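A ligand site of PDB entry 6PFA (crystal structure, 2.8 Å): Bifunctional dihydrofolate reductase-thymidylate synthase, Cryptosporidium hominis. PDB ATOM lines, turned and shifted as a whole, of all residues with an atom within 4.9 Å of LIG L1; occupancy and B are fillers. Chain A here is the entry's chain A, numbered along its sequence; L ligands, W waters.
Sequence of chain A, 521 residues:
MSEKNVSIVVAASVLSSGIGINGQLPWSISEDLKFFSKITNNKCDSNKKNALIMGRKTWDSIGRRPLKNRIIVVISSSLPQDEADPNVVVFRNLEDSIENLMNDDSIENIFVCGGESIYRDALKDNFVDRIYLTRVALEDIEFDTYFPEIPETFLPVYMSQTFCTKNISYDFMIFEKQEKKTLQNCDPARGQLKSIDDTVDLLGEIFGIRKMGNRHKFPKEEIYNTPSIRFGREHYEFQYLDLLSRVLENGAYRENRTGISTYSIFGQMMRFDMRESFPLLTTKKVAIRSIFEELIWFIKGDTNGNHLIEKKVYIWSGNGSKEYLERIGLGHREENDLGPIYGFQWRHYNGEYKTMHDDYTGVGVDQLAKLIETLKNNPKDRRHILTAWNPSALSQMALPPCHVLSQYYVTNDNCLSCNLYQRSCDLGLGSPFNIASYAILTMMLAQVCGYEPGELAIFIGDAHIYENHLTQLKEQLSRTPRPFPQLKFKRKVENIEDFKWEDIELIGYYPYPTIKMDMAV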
ATOM      1  N   ARG A 257     -25.739  20.694 -12.886  1.00  0.00           N
ATOM      2  CA  ARG A 257     -25.388  19.268 -12.874  1.00  0.00           C
ATOM      3  C   ARG A 257     -24.594  18.870 -11.645  1.00  0.00           C
ATOM      4  O   ARG A 257     -24.507  17.669 -11.339  1.00  0.00           O
ATOM      5  CB  ARG A 257     -24.595  18.930 -14.133  1.00  0.00           C
ATOM      6  CG  ARG A 257     -23.321  19.736 -14.280  1.00  0.00           C
ATOM      7  CD  ARG A 257     -22.445  19.238 -15.412  1.00  0.00           C
ATOM      8  NE  ARG A 257     -21.162  19.929 -15.425  1.00  0.00           N
ATOM      9  CZ  ARG A 257     -20.119  19.577 -14.676  1.00  0.00           C
ATOM     10  NH1 ARG A 257     -20.202  18.534 -13.862  1.00  0.00           N
ATOM     11  NH2 ARG A 257     -18.986  20.261 -14.749  1.00  0.00           N
ATOM     12  N   LYS A 284      -5.970  38.711  -5.929  1.00  0.00           N
ATOM     13  CA  LYS A 284      -5.759  37.339  -5.470  1.00  0.00           C
ATOM     14  C   LYS A 284      -4.550  36.784  -6.206  1.00  0.00           C
ATOM     15  O   LYS A 284      -4.403  37.006  -7.413  1.00  0.00           O
ATOM     16  CB  LYS A 284      -6.989  36.470  -5.733  1.00  0.00           C
ATOM     17  CG  LYS A 284      -6.776  34.996  -5.434  1.00  0.00           C
ATOM     18  CD  LYS A 284      -7.965  34.153  -5.873  1.00  0.00           C
ATOM     19  CE  LYS A 284      -8.168  34.232  -7.382  1.00  0.00           C
ATOM     20  NZ  LYS A 284      -9.163  33.230  -7.865  1.00  0.00           N
ATOM     21  N   LYS A 285      -3.684  36.086  -5.483  1.00  0.00           N
ATOM     22  CA  LYS A 285      -2.536  35.437  -6.110  1.00  0.00           C
ATOM     23  C   LYS A 285      -2.993  34.289  -6.998  1.00  0.00           C
ATOM     24  O   LYS A 285      -3.568  33.313  -6.504  1.00  0.00           O
ATOM     25  CB  LYS A 285      -1.552  34.944  -5.041  1.00  0.00           C
ATOM     26  CG  LYS A 285      -0.213  34.477  -5.599  1.00  0.00           C
ATOM     27  CD  LYS A 285       0.768  34.151  -4.494  1.00  0.00           C
ATOM     28  CE  LYS A 285       2.108  33.684  -5.052  1.00  0.00           C
ATOM     29  NZ  LYS A 285       3.140  33.510  -3.989  1.00  0.00           N
ATOM     30  N   VAL A 286      -2.769  34.416  -8.302  1.00  0.00           N
ATOM     31  CA  VAL A 286      -3.218  33.429  -9.280  1.00  0.00           C
ATOM     32  C   VAL A 286      -2.050  32.517  -9.632  1.00  0.00           C
ATOM     33  O   VAL A 286      -0.932  32.991  -9.870  1.00  0.00           O
ATOM     34  CB  VAL A 286      -3.785  34.116 -10.533  1.00  0.00           C
ATOM     35  CG1 VAL A 286      -4.412  33.086 -11.467  1.00  0.00           C
ATOM     36  CG2 VAL A 286      -4.809  35.163 -10.145  1.00  0.00           C
ATOM     37  N   ALA A 287      -2.314  31.215  -9.669  1.00  0.00           N
ATOM     38  CA  ALA A 287      -1.309  30.218 -10.017  1.00  0.00           C
ATOM     39  C   ALA A 287      -0.950  30.301 -11.498  1.00  0.00           C
ATOM     40  O   ALA A 287      -1.531  29.598 -12.330  1.00  0.00           O
ATOM     41  CB  ALA A 287      -1.793  28.818  -9.665  1.00  0.00           C
ATOM     42  N   SER A 290       0.378  26.867 -13.360  1.00  0.00           N
ATOM     43  CA  SER A 290      -0.617  25.884 -13.756  1.00  0.00           C
ATOM     44  C   SER A 290      -1.395  26.345 -14.984  1.00  0.00           C
ATOM     45  O   SER A 290      -1.792  25.506 -15.809  1.00  0.00           O
ATOM     46  CB  SER A 290      -1.579  25.608 -12.596  1.00  0.00           C
ATOM     47  OG  SER A 290      -0.861  25.225 -11.428  1.00  0.00           O
ATOM     48  N   ILE A 315      -5.681  20.468 -11.949  1.00  0.00           N
ATOM     49  CA  ILE A 315      -6.939  21.140 -12.215  1.00  0.00           C
ATOM     50  C   ILE A 315      -7.912  20.224 -12.953  1.00  0.00           C
ATOM     51  O   ILE A 315      -9.134  20.405 -12.860  1.00  0.00           O
ATOM     52  CB  ILE A 315      -6.715  22.449 -12.992  1.00  0.00           C
ATOM     53  CG1 ILE A 315      -6.086  22.180 -14.364  1.00  0.00           C
ATOM     54  CG2 ILE A 315      -5.841  23.404 -12.183  1.00  0.00           C
ATOM     55  CD1 ILE A 315      -5.994  23.409 -15.244  1.00  0.00           C
ATOM     56  N   TRP A 316      -7.407  19.229 -13.693  1.00  0.00           N
ATOM     57  CA  TRP A 316      -8.254  18.294 -14.425  1.00  0.00           C
ATOM     58  C   TRP A 316      -8.382  16.945 -13.711  1.00  0.00           C
ATOM     59  O   TRP A 316      -8.763  15.954 -14.350  1.00  0.00           O
ATOM     60  CB  TRP A 316      -7.720  18.087 -15.841  1.00  0.00           C
ATOM     61  CG  TRP A 316      -8.006  19.241 -16.758  1.00  0.00           C
ATOM     62  CD1 TRP A 316      -7.162  20.255 -17.089  1.00  0.00           C
ATOM     63  CD2 TRP A 316      -9.250  19.497 -17.433  1.00  0.00           C
ATOM     64  NE1 TRP A 316      -7.788  21.127 -17.950  1.00  0.00           N
ATOM     65  CE2 TRP A 316      -9.069  20.691 -18.173  1.00  0.00           C
ATOM     66  CE3 TRP A 316     -10.475  18.848 -17.491  1.00  0.00           C
ATOM     67  CZ2 TRP A 316     -10.077  21.230 -18.967  1.00  0.00           C
ATOM     68  CZ3 TRP A 316     -11.482  19.388 -18.285  1.00  0.00           C
ATOM     69  CH2 TRP A 316     -11.277  20.561 -19.006  1.00  0.00           C
ATOM     70  N   ASN A 319     -12.550  16.183 -13.057  1.00  0.00           N
ATOM     71  CA  ASN A 319     -13.274  15.746 -14.246  1.00  0.00           C
ATOM     72  C   ASN A 319     -12.572  14.610 -14.975  1.00  0.00           C
ATOM     73  O   ASN A 319     -12.998  14.251 -16.083  1.00  0.00           O
ATOM     74  CB  ASN A 319     -13.479  16.934 -15.193  1.00  0.00           C
ATOM     75  CG  ASN A 319     -14.072  18.139 -14.490  1.00  0.00           C
ATOM     76  OD1 ASN A 319     -13.352  19.024 -14.039  1.00  0.00           O
ATOM     77  ND2 ASN A 319     -15.395  18.176 -14.385  1.00  0.00           N
ATOM     78  N   LEU A 399     -16.003  16.560 -20.533  1.00  0.00           N
ATOM     79  CA  LEU A 399     -16.699  17.803 -20.235  1.00  0.00           C
ATOM     80  C   LEU A 399     -16.681  18.679 -21.477  1.00  0.00           C
ATOM     81  O   LEU A 399     -15.611  18.902 -22.059  1.00  0.00           O
ATOM     82  CB  LEU A 399     -16.053  18.513 -19.041  1.00  0.00           C
ATOM     83  CG  LEU A 399     -16.806  19.702 -18.446  1.00  0.00           C
ATOM     84  CD1 LEU A 399     -18.182  19.277 -17.950  1.00  0.00           C
ATOM     85  CD2 LEU A 399     -16.007  20.342 -17.328  1.00  0.00           C
ATOM     86  N   ASP A 426     -17.068  29.867 -14.515  1.00  0.00           N
ATOM     87  CA  ASP A 426     -16.872  29.834 -13.070  1.00  0.00           C
ATOM     88  C   ASP A 426     -16.062  31.062 -12.693  1.00  0.00           C
ATOM     89  O   ASP A 426     -14.838  31.087 -12.832  1.00  0.00           O
ATOM     90  CB  ASP A 426     -16.168  28.549 -12.657  1.00  0.00           C
ATOM     91  CG  ASP A 426     -15.950  28.443 -11.155  1.00  0.00           C
ATOM     92  OD1 ASP A 426     -16.349  29.365 -10.411  1.00  0.00           O
ATOM     93  OD2 ASP A 426     -15.363  27.426 -10.721  1.00  0.00           O
ATOM     94  N   LEU A 429     -12.995  30.474 -10.094  1.00  0.00           N
ATOM     95  CA  LEU A 429     -11.823  29.674 -10.445  1.00  0.00           C
ATOM     96  C   LEU A 429     -11.492  29.744 -11.927  1.00  0.00           C
ATOM     97  O   LEU A 429     -10.384  30.126 -12.285  1.00  0.00           O
ATOM     98  CB  LEU A 429     -12.046  28.213 -10.016  1.00  0.00           C
ATOM     99  CG  LEU A 429     -12.249  27.935  -8.535  1.00  0.00           C
ATOM    100  CD1 LEU A 429     -12.407  26.442  -8.299  1.00  0.00           C
ATOM    101  CD2 LEU A 429     -11.084  28.493  -7.721  1.00  0.00           C
ATOM    102  N   GLY A 430     -12.435  29.370 -12.798  1.00  0.00           N
ATOM    103  CA  GLY A 430     -12.122  29.295 -14.214  1.00  0.00           C
ATOM    104  C   GLY A 430     -11.826  30.652 -14.828  1.00  0.00           C
ATOM    105  O   GLY A 430     -10.940  30.778 -15.675  1.00  0.00           O
ATOM    106  N   PHE A 433      -8.353  32.016 -14.604  1.00  0.00           N
ATOM    107  CA  PHE A 433      -7.526  31.178 -15.462  1.00  0.00           C
ATOM    108  C   PHE A 433      -7.772  31.506 -16.933  1.00  0.00           C
ATOM    109  O   PHE A 433      -6.817  31.626 -17.710  1.00  0.00           O
ATOM    110  CB  PHE A 433      -7.809  29.709 -15.187  1.00  0.00           C
ATOM    111  CG  PHE A 433      -7.019  29.147 -14.039  1.00  0.00           C
ATOM    112  CD1 PHE A 433      -7.080  29.729 -12.781  1.00  0.00           C
ATOM    113  CD2 PHE A 433      -6.226  28.026 -14.202  1.00  0.00           C
ATOM    114  CE1 PHE A 433      -6.363  29.225 -11.721  1.00  0.00           C
ATOM    115  CE2 PHE A 433      -5.488  27.509 -13.146  1.00  0.00           C
ATOM    116  CZ  PHE A 433      -5.563  28.106 -11.903  1.00  0.00           C
ATOM    117  N   TYR A 466     -20.508  29.991  -7.740  1.00  0.00           N
ATOM    118  CA  TYR A 466     -20.921  28.866  -6.903  1.00  0.00           C
ATOM    119  C   TYR A 466     -21.147  29.334  -5.472  1.00  0.00           C
ATOM    120  O   TYR A 466     -20.425  30.192  -4.969  1.00  0.00           O
ATOM    121  CB  TYR A 466     -19.886  27.756  -6.947  1.00  0.00           C
ATOM    122  CG  TYR A 466     -19.880  27.000  -8.264  1.00  0.00           C
ATOM    123  CD1 TYR A 466     -19.147  27.454  -9.348  1.00  0.00           C
ATOM    124  CD2 TYR A 466     -20.644  25.846  -8.422  1.00  0.00           C
ATOM    125  CE1 TYR A 466     -19.153  26.769 -10.555  1.00  0.00           C
ATOM    126  CE2 TYR A 466     -20.653  25.160  -9.620  1.00  0.00           C
ATOM    127  CZ  TYR A 466     -19.907  25.622 -10.686  1.00  0.00           C
ATOM    128  OH  TYR A 466     -19.924  24.944 -11.876  1.00  0.00           O
ATOM    129  N   THR A 514      -3.384  34.546  -1.496  1.00  0.00           N
ATOM    130  CA  THR A 514      -4.211  33.597  -2.232  1.00  0.00           C
ATOM    131  C   THR A 514      -5.484  33.267  -1.449  1.00  0.00           C
ATOM    132  O   THR A 514      -5.518  33.353  -0.214  1.00  0.00           O
ATOM    133  CB  THR A 514      -3.437  32.323  -2.535  1.00  0.00           C
ATOM    134  OG1 THR A 514      -4.292  31.380  -3.185  1.00  0.00           O
ATOM    135  CG2 THR A 514      -2.881  31.710  -1.258  1.00  0.00           C
ATOM    136  N   ILE A 515      -6.530  32.913  -2.187  1.00  0.00           N
ATOM    137  CA  ILE A 515      -7.833  32.593  -1.620  1.00  0.00           C
ATOM    138  C   ILE A 515      -8.219  31.197  -2.092  1.00  0.00           C
ATOM    139  O   ILE A 515      -8.294  30.943  -3.299  1.00  0.00           O
ATOM    140  CB  ILE A 515      -8.896  33.618  -2.015  1.00  0.00           C
ATOM    141  CG1 ILE A 515      -8.430  35.029  -1.662  1.00  0.00           C
ATOM    142  CG2 ILE A 515     -10.223  33.310  -1.327  1.00  0.00           C
ATOM    143  CD1 ILE A 515      -9.415  36.124  -2.041  1.00  0.00           C
ATOM    144  N   MET A 517     -10.544  28.105  -2.932  1.00  0.00           N
ATOM    145  CA  MET A 517     -11.909  27.874  -3.386  1.00  0.00           C
ATOM    146  C   MET A 517     -11.994  26.480  -3.997  1.00  0.00           C
ATOM    147  O   MET A 517     -11.191  26.137  -4.865  1.00  0.00           O
ATOM    148  CB  MET A 517     -12.370  28.929  -4.392  1.00  0.00           C
ATOM    149  CG  MET A 517     -12.717  30.271  -3.774  1.00  0.00           C
ATOM    150  SD  MET A 517     -13.065  31.543  -5.008  1.00  0.00           S
ATOM    151  CE  MET A 517     -11.412  31.994  -5.510  1.00  0.00           C
ATOM    152  N   MET A 519     -13.396  23.384  -6.221  1.00  0.00           N
ATOM    153  CA  MET A 519     -14.034  23.208  -7.515  1.00  0.00           C
ATOM    154  C   MET A 519     -15.219  22.251  -7.400  1.00  0.00           C
ATOM    155  O   MET A 519     -15.159  21.252  -6.689  1.00  0.00           O
ATOM    156  CB  MET A 519     -13.030  22.667  -8.536  1.00  0.00           C
ATOM    157  CG  MET A 519     -13.638  22.345  -9.896  1.00  0.00           C
ATOM    158  SD  MET A 519     -12.563  21.358 -10.961  1.00  0.00           S
ATOM    159  CE  MET A 519     -12.230  19.953  -9.896  1.00  0.00           C
ATOM    160  N   ALA A 520     -16.284  22.573  -8.118  1.00  0.00           N
ATOM    161  CA  ALA A 520     -17.461  21.714  -8.186  1.00  0.00           C
ATOM    162  C   ALA A 520     -17.278  20.662  -9.276  1.00  0.00           C
ATOM    163  O   ALA A 520     -17.010  21.009 -10.434  1.00  0.00           O
ATOM    164  CB  ALA A 520     -18.722  22.529  -8.441  1.00  0.00           C
HETATM  165  C1  LIG L   1      -9.077  26.169 -12.043  1.00  0.00           C
HETATM  166  C2  LIG L   1      -9.134  25.092 -11.115  1.00  0.00           C
HETATM  167  C3  LIG L   1      -7.556  28.500  -7.682  1.00  0.00           C
HETATM  168  C4  LIG L   1      -4.014  26.943  -7.690  1.00  0.00           C
HETATM  169  C5  LIG L   1     -14.012  22.866 -14.423  1.00  0.00           C
HETATM  170  C6  LIG L   1      -9.734  23.880 -11.525  1.00  0.00           C
HETATM  171  C7  LIG L   1     -10.254  23.735 -12.824  1.00  0.00           C
HETATM  172  C8  LIG L   1      -8.598  25.187  -9.717  1.00  0.00           C
HETATM  173  C9  LIG L   1      -6.946  26.121  -8.170  1.00  0.00           C
HETATM  174  C10 LIG L   1      -6.524  27.536  -7.801  1.00  0.00           C
HETATM  175  C11 LIG L   1      -5.166  27.918  -7.585  1.00  0.00           C
HETATM  176  C12 LIG L   1      -4.892  29.264  -7.238  1.00  0.00           C
HETATM  177  C13 LIG L   1      -5.928  30.215  -7.121  1.00  0.00           C
HETATM  178  C14 LIG L   1     -13.177  23.945 -14.234  1.00  0.00           C
HETATM  179  C15 LIG L   1      -7.258  29.833  -7.348  1.00  0.00           C
HETATM  180  C16 LIG L   1     -13.655  25.010 -13.335  1.00  0.00           C
HETATM  181  C17 LIG L   1     -15.643  23.671 -13.066  1.00  0.00           C
HETATM  182  C18 LIG L   1     -11.999  23.714 -15.018  1.00  0.00           C
HETATM  183  C19 LIG L   1     -12.163  22.502 -15.655  1.00  0.00           C
HETATM  184  C20 LIG L   1     -10.785  24.607 -15.126  1.00  0.00           C
HETATM  185  C21 LIG L   1     -10.196  24.802 -13.742  1.00  0.00           C
HETATM  186  C22 LIG L   1      -9.605  26.020 -13.345  1.00  0.00           C
HETATM  187  N1  LIG L   1     -15.262  22.703 -13.854  1.00  0.00           N
HETATM  188  N2  LIG L   1     -14.878  24.814 -12.790  1.00  0.00           N
HETATM  189  N3  LIG L   1     -13.397  21.998 -15.282  1.00  0.00           N
HETATM  190  N4  LIG L   1     -16.839  23.696 -12.393  1.00  0.00           N
HETATM  191  N5  LIG L   1      -7.541  25.984  -9.497  1.00  0.00           N
HETATM  192  O1  LIG L   1     -12.994  26.027 -13.091  1.00  0.00           O
HETATM  193  O2  LIG L   1      -9.126  24.533  -8.819  1.00  0.00           O
HETATM  194  O3  LIG L   1      -3.817  26.445  -8.941  1.00  0.00           O
HETATM  195  O4  LIG L   1      -3.302  26.637  -6.733  1.00  0.00           O
HETATM  196  N1  LG2 L   2     -15.204  26.358 -16.366  1.00  0.00           N
HETATM  197  C1  LG2 L   2     -14.754  27.616 -16.648  1.00  0.00           C
HETATM  198  N2  LG2 L   2     -13.669  27.794 -17.432  1.00  0.00           N
HETATM  199  C2  LG2 L   2     -12.994  26.742 -17.949  1.00  0.00           C
HETATM  200  C3  LG2 L   2     -13.436  25.434 -17.658  1.00  0.00           C
HETATM  201  C4  LG2 L   2     -14.520  25.278 -16.871  1.00  0.00           C
HETATM  202  O1  LG2 L   2     -15.294  28.632 -16.232  1.00  0.00           O
HETATM  203  O2  LG2 L   2     -12.020  26.923 -18.648  1.00  0.00           O
HETATM  204  F1  LG2 L   2     -12.793  24.358 -18.157  1.00  0.00           F
HETATM  205  C5  LG2 L   2     -16.373  25.991 -15.534  1.00  0.00           C
HETATM  206  C6  LG2 L   2     -17.686  26.732 -15.859  1.00  0.00           C
HETATM  207  C7  LG2 L   2     -18.707  25.791 -15.182  1.00  0.00           C
HETATM  208  C8  LG2 L   2     -18.116  24.391 -15.472  1.00  0.00           C
HETATM  209  O3  LG2 L   2     -18.729  26.008 -13.768  1.00  0.00           O
HETATM  210  O4  LG2 L   2     -16.717  24.609 -15.815  1.00  0.00           O
HETATM  211  C9  LG2 L   2     -18.882  23.698 -16.604  1.00  0.00           C
HETATM  212  O5  LG2 L   2     -20.131  23.232 -16.104  1.00  0.00           O
HETATM  213  P1  LG2 L   2     -21.142  22.993 -17.325  1.00  0.00           P
HETATM  214  O6  LG2 L   2     -22.379  22.356 -16.825  1.00  0.00           O
HETATM  215  O7  LG2 L   2     -20.456  22.016 -18.413  1.00  0.00           O
HETATM  216  O8  LG2 L   2     -21.515  24.392 -18.017  1.00  0.00           O
HETATM  217  O   HOH W   1      -8.932  31.484  -9.807  1.00  0.00           O
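An oxygen (O6) of LG2 L2 is in salt-bridge range of the guanidinium group (NE) of Arg 257, 3.1 Å away. OD1 of Asn 319 is in hydrogen-bond range of N3 of LIG L1. OD2 of Asp 426 is in hydrogen-bond range of N2 of LIG L1. N of Gly 430 lies within hydrogen-bond range of O1 of LIG L1 (3.4 Å). An oxygen (O1) of LG2 L2 lies within hydrogen-bond range of the backbone NH (N) of Asp 426. The side-chain hydroxyl of Tyr 466 lies within hydrogen-bond range of a nitrogen (N4) of LIG L1 (3.4 Å). O of Ala 520 is in hydrogen-bond range of N4 of LIG L1 (3.3 Å). OH of Tyr 466 is in hydrogen-bond range of O3 of LG2 L2, at 2.5 Å.
Water W1 lies within hydrogen-bond range of the side-chain amino group of Lys 284 (2.6 Å) and the backbone carbonyl oxygen of Leu 429 (3.2 Å).
Merely in contact with LIG L1: Ala 287, Ile 315, Leu 429, Leu 399, Phe 433, Met 519, Lys 284, Lys 285 and Trp 316. Hydrophobic or aromatic side chains within 4 Å of LIG L1: Ala 287, Ile 315, Trp 316, Leu 399, Leu 429, Phe 433 and Met 519.
O3 of LG2 L2 is in hydrogen-bond range of N4 of LIG L1, at 3.3 Å.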
